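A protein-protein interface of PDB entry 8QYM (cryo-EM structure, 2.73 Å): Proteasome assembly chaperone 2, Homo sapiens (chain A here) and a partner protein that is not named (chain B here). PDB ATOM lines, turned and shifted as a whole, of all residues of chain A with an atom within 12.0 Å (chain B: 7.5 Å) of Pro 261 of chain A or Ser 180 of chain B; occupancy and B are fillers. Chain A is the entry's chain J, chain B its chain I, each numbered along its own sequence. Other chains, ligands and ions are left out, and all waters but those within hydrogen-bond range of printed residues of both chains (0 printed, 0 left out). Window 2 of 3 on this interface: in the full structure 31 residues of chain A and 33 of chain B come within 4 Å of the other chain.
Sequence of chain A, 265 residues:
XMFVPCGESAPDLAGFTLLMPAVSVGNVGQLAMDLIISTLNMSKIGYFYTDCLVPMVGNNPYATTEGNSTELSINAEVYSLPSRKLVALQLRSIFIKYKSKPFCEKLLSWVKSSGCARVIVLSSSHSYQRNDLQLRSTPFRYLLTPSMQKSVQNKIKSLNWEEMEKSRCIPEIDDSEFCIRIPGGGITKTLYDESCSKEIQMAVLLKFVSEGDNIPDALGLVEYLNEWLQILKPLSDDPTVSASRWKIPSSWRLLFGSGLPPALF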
ATOM      1  N   ARG A 253     -11.325  -7.034 -22.344  1.00  0.00           N
ATOM      2  CA  ARG A 253     -11.716  -7.367 -20.980  1.00  0.00           C
ATOM      3  C   ARG A 253     -11.659  -8.862 -20.694  1.00  0.00           C
ATOM      4  O   ARG A 253     -10.975  -9.283 -19.757  1.00  0.00           O
ATOM      5  CB  ARG A 253     -13.121  -6.823 -20.695  1.00  0.00           C
ATOM      6  CG  ARG A 253     -13.412  -6.633 -19.219  1.00  0.00           C
ATOM      7  CD  ARG A 253     -14.555  -5.662 -18.997  1.00  0.00           C
ATOM      8  NE  ARG A 253     -15.814  -6.161 -19.536  1.00  0.00           N
ATOM      9  CZ  ARG A 253     -16.689  -6.881 -18.849  1.00  0.00           C
ATOM     10  NH1 ARG A 253     -16.469  -7.220 -17.590  1.00  0.00           N
ATOM     11  NH2 ARG A 253     -17.816  -7.270 -19.439  1.00  0.00           N
ATOM     12  N   LEU A 254     -12.361  -9.683 -21.470  1.00  0.00           N
ATOM     13  CA  LEU A 254     -12.427 -11.124 -21.230  1.00  0.00           C
ATOM     14  C   LEU A 254     -11.956 -11.831 -22.495  1.00  0.00           C
ATOM     15  O   LEU A 254     -12.763 -12.198 -23.351  1.00  0.00           O
ATOM     16  CB  LEU A 254     -13.842 -11.549 -20.845  1.00  0.00           C
ATOM     17  CG  LEU A 254     -14.461 -10.865 -19.626  1.00  0.00           C
ATOM     18  CD1 LEU A 254     -15.973 -10.856 -19.737  1.00  0.00           C
ATOM     19  CD2 LEU A 254     -14.024 -11.545 -18.342  1.00  0.00           C
ATOM     20  N   PHE A 256     -10.257 -14.733 -22.543  1.00  0.00           N
ATOM     21  CA  PHE A 256     -10.189 -16.174 -22.367  1.00  0.00           C
ATOM     22  C   PHE A 256     -11.536 -16.820 -22.085  1.00  0.00           C
ATOM     23  O   PHE A 256     -11.622 -18.053 -22.094  1.00  0.00           O
ATOM     24  CB  PHE A 256      -9.216 -16.530 -21.231  1.00  0.00           C
ATOM     25  CG  PHE A 256      -7.794 -16.706 -21.682  1.00  0.00           C
ATOM     26  CD1 PHE A 256      -7.368 -17.907 -22.221  1.00  0.00           C
ATOM     27  CD2 PHE A 256      -6.883 -15.671 -21.564  1.00  0.00           C
ATOM     28  CE1 PHE A 256      -6.062 -18.072 -22.636  1.00  0.00           C
ATOM     29  CE2 PHE A 256      -5.575 -15.833 -21.977  1.00  0.00           C
ATOM     30  CZ  PHE A 256      -5.166 -17.034 -22.513  1.00  0.00           C
ATOM     31  N   GLY A 257     -12.584 -16.037 -21.838  1.00  0.00           N
ATOM     32  CA  GLY A 257     -13.903 -16.593 -21.612  1.00  0.00           C
ATOM     33  C   GLY A 257     -14.577 -16.081 -20.357  1.00  0.00           C
ATOM     34  O   GLY A 257     -14.319 -14.957 -19.918  1.00  0.00           O
ATOM     35  N   SER A 258     -15.444 -16.901 -19.771  1.00  0.00           N
ATOM     36  CA  SER A 258     -16.175 -16.537 -18.567  1.00  0.00           C
ATOM     37  C   SER A 258     -15.398 -16.990 -17.331  1.00  0.00           C
ATOM     38  O   SER A 258     -14.229 -17.377 -17.409  1.00  0.00           O
ATOM     39  CB  SER A 258     -17.581 -17.128 -18.606  1.00  0.00           C
ATOM     40  OG  SER A 258     -18.302 -16.647 -19.726  1.00  0.00           O
ATOM     41  N   GLY A 259     -16.048 -16.948 -16.169  1.00  0.00           N
ATOM     42  CA  GLY A 259     -15.402 -17.275 -14.918  1.00  0.00           C
ATOM     43  C   GLY A 259     -15.288 -18.768 -14.677  1.00  0.00           C
ATOM     44  O   GLY A 259     -15.661 -19.603 -15.500  1.00  0.00           O
ATOM     45  N   LEU A 260     -14.756 -19.101 -13.501  1.00  0.00           N
ATOM     46  CA  LEU A 260     -14.454 -20.468 -13.088  1.00  0.00           C
ATOM     47  C   LEU A 260     -15.667 -21.100 -12.413  1.00  0.00           C
ATOM     48  O   LEU A 260     -16.226 -20.509 -11.483  1.00  0.00           O
ATOM     49  CB  LEU A 260     -13.269 -20.486 -12.134  1.00  0.00           C
ATOM     50  CG  LEU A 260     -12.618 -21.836 -11.839  1.00  0.00           C
ATOM     51  CD1 LEU A 260     -12.069 -22.456 -13.108  1.00  0.00           C
ATOM     52  CD2 LEU A 260     -11.522 -21.673 -10.804  1.00  0.00           C
ATOM     53  N   PRO A 261     -16.103 -22.283 -12.854  1.00  0.00           N
ATOM     54  CA  PRO A 261     -17.238 -22.931 -12.199  1.00  0.00           C
ATOM     55  C   PRO A 261     -16.875 -23.360 -10.789  1.00  0.00           C
ATOM     56  O   PRO A 261     -15.700 -23.637 -10.491  1.00  0.00           O
ATOM     57  CB  PRO A 261     -17.520 -24.148 -13.100  1.00  0.00           C
ATOM     58  CG  PRO A 261     -16.813 -23.863 -14.384  1.00  0.00           C
ATOM     59  CD  PRO A 261     -15.622 -23.048 -14.014  1.00  0.00           C
ATOM     60  N   PRO A 262     -17.848 -23.432  -9.888  1.00  0.00           N
ATOM     61  CA  PRO A 262     -17.561 -23.829  -8.506  1.00  0.00           C
ATOM     62  C   PRO A 262     -17.440 -25.342  -8.368  1.00  0.00           C
ATOM     63  O   PRO A 262     -17.694 -26.107  -9.299  1.00  0.00           O
ATOM     64  CB  PRO A 262     -18.769 -23.300  -7.718  1.00  0.00           C
ATOM     65  CG  PRO A 262     -19.634 -22.559  -8.718  1.00  0.00           C
ATOM     66  CD  PRO A 262     -19.261 -23.070 -10.068  1.00  0.00           C
ATOM     67  N   ALA A 263     -17.035 -25.757  -7.166  1.00  0.00           N
ATOM     68  CA  ALA A 263     -16.917 -27.171  -6.801  1.00  0.00           C
ATOM     69  C   ALA A 263     -15.942 -27.912  -7.712  1.00  0.00           C
ATOM     70  O   ALA A 263     -16.155 -29.072  -8.067  1.00  0.00           O
ATOM     71  CB  ALA A 263     -18.284 -27.859  -6.802  1.00  0.00           C
ATOM     72  N   LEU A 264     -14.869 -27.242  -8.092  1.00  0.00           N
ATOM     73  CA  LEU A 264     -13.860 -27.862  -8.945  1.00  0.00           C
ATOM     74  C   LEU A 264     -12.453 -27.754  -8.379  1.00  0.00           C
ATOM     75  O   LEU A 264     -11.666 -28.693  -8.523  1.00  0.00           O
ATOM     76  CB  LEU A 264     -13.911 -27.236 -10.346  1.00  0.00           C
ATOM     77  CG  LEU A 264     -13.157 -27.962 -11.458  1.00  0.00           C
ATOM     78  CD1 LEU A 264     -13.726 -29.347 -11.665  1.00  0.00           C
ATOM     79  CD2 LEU A 264     -13.224 -27.165 -12.744  1.00  0.00           C
ATOM     80  N   PHE A 265     -12.119 -26.643  -7.734  1.00  0.00           N
ATOM     81  CA  PHE A 265     -10.777 -26.438  -7.202  1.00  0.00           C
ATOM     82  C   PHE A 265     -10.802 -26.332  -5.682  1.00  0.00           C
ATOM     83  O   PHE A 265     -11.156 -25.292  -5.128  1.00  0.00           O
ATOM     84  CB  PHE A 265     -10.147 -25.184  -7.808  1.00  0.00           C
ATOM     85  CG  PHE A 265      -9.595 -25.389  -9.187  1.00  0.00           C
ATOM     86  CD1 PHE A 265      -8.291 -25.813  -9.370  1.00  0.00           C
ATOM     87  CD2 PHE A 265     -10.381 -25.161 -10.302  1.00  0.00           C
ATOM     88  CE1 PHE A 265      -7.783 -26.003 -10.639  1.00  0.00           C
ATOM     89  CE2 PHE A 265      -9.878 -25.350 -11.573  1.00  0.00           C
ATOM     90  CZ  PHE A 265      -8.578 -25.772 -11.741  1.00  0.00           C
ATOM     91  N   TYR B 175     -22.946 -16.102 -23.621  1.00  0.00           N
ATOM     92  CA  TYR B 175     -22.750 -14.863 -22.885  1.00  0.00           C
ATOM     93  C   TYR B 175     -21.377 -14.845 -22.224  1.00  0.00           C
ATOM     94  O   TYR B 175     -20.871 -15.877 -21.778  1.00  0.00           O
ATOM     95  CB  TYR B 175     -23.844 -14.701 -21.830  1.00  0.00           C
ATOM     96  CG  TYR B 175     -24.119 -13.270 -21.435  1.00  0.00           C
ATOM     97  CD1 TYR B 175     -24.730 -12.391 -22.316  1.00  0.00           C
ATOM     98  CD2 TYR B 175     -23.774 -12.801 -20.177  1.00  0.00           C
ATOM     99  CE1 TYR B 175     -24.985 -11.084 -21.957  1.00  0.00           C
ATOM    100  CE2 TYR B 175     -24.024 -11.496 -19.809  1.00  0.00           C
ATOM    101  CZ  TYR B 175     -24.630 -10.643 -20.702  1.00  0.00           C
ATOM    102  OH  TYR B 175     -24.882  -9.340 -20.340  1.00  0.00           O
ATOM    103  N   THR B 177     -19.137 -13.095 -19.175  1.00  0.00           N
ATOM    104  CA  THR B 177     -19.238 -12.376 -17.915  1.00  0.00           C
ATOM    105  C   THR B 177     -18.080 -12.785 -17.019  1.00  0.00           C
ATOM    106  O   THR B 177     -17.468 -13.839 -17.208  1.00  0.00           O
ATOM    107  CB  THR B 177     -20.577 -12.645 -17.218  1.00  0.00           C
ATOM    108  OG1 THR B 177     -20.581 -12.026 -15.927  1.00  0.00           O
ATOM    109  CG2 THR B 177     -20.800 -14.140 -17.058  1.00  0.00           C
ATOM    110  N   SER B 178     -17.784 -11.935 -16.036  1.00  0.00           N
ATOM    111  CA  SER B 178     -16.721 -12.244 -15.088  1.00  0.00           C
ATOM    112  C   SER B 178     -17.111 -13.355 -14.125  1.00  0.00           C
ATOM    113  O   SER B 178     -16.230 -13.971 -13.518  1.00  0.00           O
ATOM    114  CB  SER B 178     -16.331 -10.989 -14.306  1.00  0.00           C
ATOM    115  OG  SER B 178     -17.433 -10.486 -13.572  1.00  0.00           O
ATOM    116  N   GLU B 179     -18.404 -13.623 -13.972  1.00  0.00           N
ATOM    117  CA  GLU B 179     -18.883 -14.697 -13.118  1.00  0.00           C
ATOM    118  C   GLU B 179     -18.982 -15.987 -13.929  1.00  0.00           C
ATOM    119  O   GLU B 179     -18.506 -16.072 -15.064  1.00  0.00           O
ATOM    120  CB  GLU B 179     -20.224 -14.314 -12.495  1.00  0.00           C
ATOM    121  CG  GLU B 179     -20.223 -12.966 -11.800  1.00  0.00           C
ATOM    122  CD  GLU B 179     -19.423 -12.976 -10.513  1.00  0.00           C
ATOM    123  OE1 GLU B 179     -19.468 -13.997  -9.793  1.00  0.00           O
ATOM    124  OE2 GLU B 179     -18.751 -11.967 -10.220  1.00  0.00           O
ATOM    125  N   SER B 180     -19.603 -17.009 -13.353  1.00  0.00           N
ATOM    126  CA  SER B 180     -19.832 -18.264 -14.051  1.00  0.00           C
ATOM    127  C   SER B 180     -21.194 -18.236 -14.729  1.00  0.00           C
ATOM    128  O   SER B 180     -22.157 -17.683 -14.190  1.00  0.00           O
ATOM    129  CB  SER B 180     -19.749 -19.444 -13.082  1.00  0.00           C
ATOM    130  OG  SER B 180     -19.662 -20.672 -13.783  1.00  0.00           O
ATOM    131  N   THR B 181     -21.269 -18.837 -15.919  1.00  0.00           N
ATOM    132  CA  THR B 181     -22.519 -18.835 -16.673  1.00  0.00           C
ATOM    133  C   THR B 181     -23.613 -19.646 -15.990  1.00  0.00           C
ATOM    134  O   THR B 181     -24.788 -19.488 -16.338  1.00  0.00           O
ATOM    135  CB  THR B 181     -22.288 -19.370 -18.087  1.00  0.00           C
ATOM    136  OG1 THR B 181     -21.718 -20.683 -18.019  1.00  0.00           O
ATOM    137  CG2 THR B 181     -21.352 -18.452 -18.859  1.00  0.00           C
ATOM    138  N   GLY B 182     -23.259 -20.504 -15.035  1.00  0.00           N
ATOM    139  CA  GLY B 182     -24.256 -21.261 -14.303  1.00  0.00           C
ATOM    140  C   GLY B 182     -24.955 -20.502 -13.198  1.00  0.00           C
ATOM    141  O   GLY B 182     -25.986 -20.967 -12.704  1.00  0.00           O
ATOM    142  N   SER B 183     -24.422 -19.351 -12.797  1.00  0.00           N
ATOM    143  CA  SER B 183     -25.029 -18.523 -11.765  1.00  0.00           C
ATOM    144  C   SER B 183     -25.918 -17.424 -12.331  1.00  0.00           C
ATOM    145  O   SER B 183     -26.512 -16.667 -11.558  1.00  0.00           O
ATOM    146  CB  SER B 183     -23.942 -17.900 -10.885  1.00  0.00           C
ATOM    147  OG  SER B 183     -23.112 -17.035 -11.639  1.00  0.00           O
ATOM    148  N   LEU B 184     -26.020 -17.317 -13.648  1.00  0.00           N
ATOM    149  CA  LEU B 184     -26.838 -16.281 -14.267  1.00  0.00           C
ATOM    150  C   LEU B 184     -28.297 -16.721 -14.301  1.00  0.00           C
ATOM    151  O   LEU B 184     -28.593 -17.827 -14.765  1.00  0.00           O
ATOM    152  CB  LEU B 184     -26.348 -15.988 -15.680  1.00  0.00           C
ATOM    153  CG  LEU B 184     -24.980 -15.317 -15.804  1.00  0.00           C
ATOM    154  CD1 LEU B 184     -24.574 -15.199 -17.262  1.00  0.00           C
ATOM    155  CD2 LEU B 184     -24.991 -13.952 -15.140  1.00  0.00           C
ATOM    156  N   PRO B 185     -29.230 -15.898 -13.819  1.00  0.00           N
ATOM    157  CA  PRO B 185     -30.648 -16.270 -13.898  1.00  0.00           C
ATOM    158  C   PRO B 185     -31.196 -16.129 -15.310  1.00  0.00           C
ATOM    159  O   PRO B 185     -31.412 -15.013 -15.794  1.00  0.00           O
ATOM    160  CB  PRO B 185     -31.321 -15.291 -12.930  1.00  0.00           C
ATOM    161  CG  PRO B 185     -30.424 -14.103 -12.918  1.00  0.00           C
ATOM    162  CD  PRO B 185     -29.026 -14.615 -13.124  1.00  0.00           C
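The side-chain hydroxyl (OG) of Ser 258 of chain A sits at hydrogen-bond distance from the backbone carbonyl oxygen (O) of Tyr 175 of chain B (3.4 Å).
N of Gly 259 of chain A lies within hydrogen-bond range of O of Glu 179 of chain B (2.8 Å).
The side-chain hydroxyl (OG1) of Thr 177 of chain B sits close to the backbone NH (N) of Glu 179 of chain B (3.3 Å).
The backbone carbonyl oxygen of Ser 180 of chain B sits at hydrogen-bond distance from the side-chain hydroxyl of Ser 183 of chain B (2.8 Å).
Among the printed residues, merely in contact across the chains: Ser 258 of chain A with Thr 177 of chain B (3.3 Å), Gly 259 of chain A with Thr 177 of chain B (3.6 Å), Ser 258 of chain A with Thr 181 of chain B (3.6 Å), Pro 261 of chain A with Ser 180 of chain B (3.7 Å), Gly 259 of chain A with Ser 178 of chain B (3.7 Å), Ser 258 of chain A with Glu 179 of chain B (3.8 Å) and Leu 254 of chain A with Thr 177 of chain B (3.9 Å).
Of the printed residues of chain B, Leu 254 of chain A touches Thr 177 (3.9 Å).
Printed residues of chain B within 4 Å of Ser 258 of chain A: Tyr 175 (3.4 Å), Thr 177 (3.3 Å), Glu 179 (3.8 Å) and Thr 181 (3.6 Å).
Of the printed residues of chain B, Gly 259 of chain A touches Thr 177 (3.6 Å), Ser 178 (3.7 Å) and Glu 179 (2.8 Å).
Of chain B, only Ser 180 comes within 4 Å of Pro 261 of chain A.
Leu 264 of chain A touches none of the printed residues of chain B.
Phe 265 of chain A touches none of the printed residues of chain B.
Of the printed residues of chain A, Tyr 175 of chain B touches Ser 258.
Thr 177 of chain B touches just these residues of chain A: Leu 254 (3.9 Å), Ser 258 (3.3 Å) and Gly 259 (3.6 Å).
Of chain A, only Gly 259 (3.7 Å) comes within 4 Å of Ser 178 of chain B.
Glu 179 of chain B touches two residues of chain A.
Of chain A, only Ser 258 (3.6 Å) comes within 4 Å of Thr 181 of chain B.
The nearest residue of chain B that does not touch Pro 261 of chain A is Thr 181 of chain B (6.8 Å).
Of the 10 printed residues of chain B, 6 touch a printed residue of chain A.
Of the 12 printed residues of chain A, 4 touch a printed residue of chain B.
Printed residues of chain A that touch a printed residue of chain B: Leu 254, Ser 258, Gly 259 and Pro 261.
Among the printed residues, 9 pairs touch across the chains.
Among the printed residues, no Asp or Glu carboxylate lies within 4 Å of a Lys or Arg side-chain nitrogen of the other chain.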
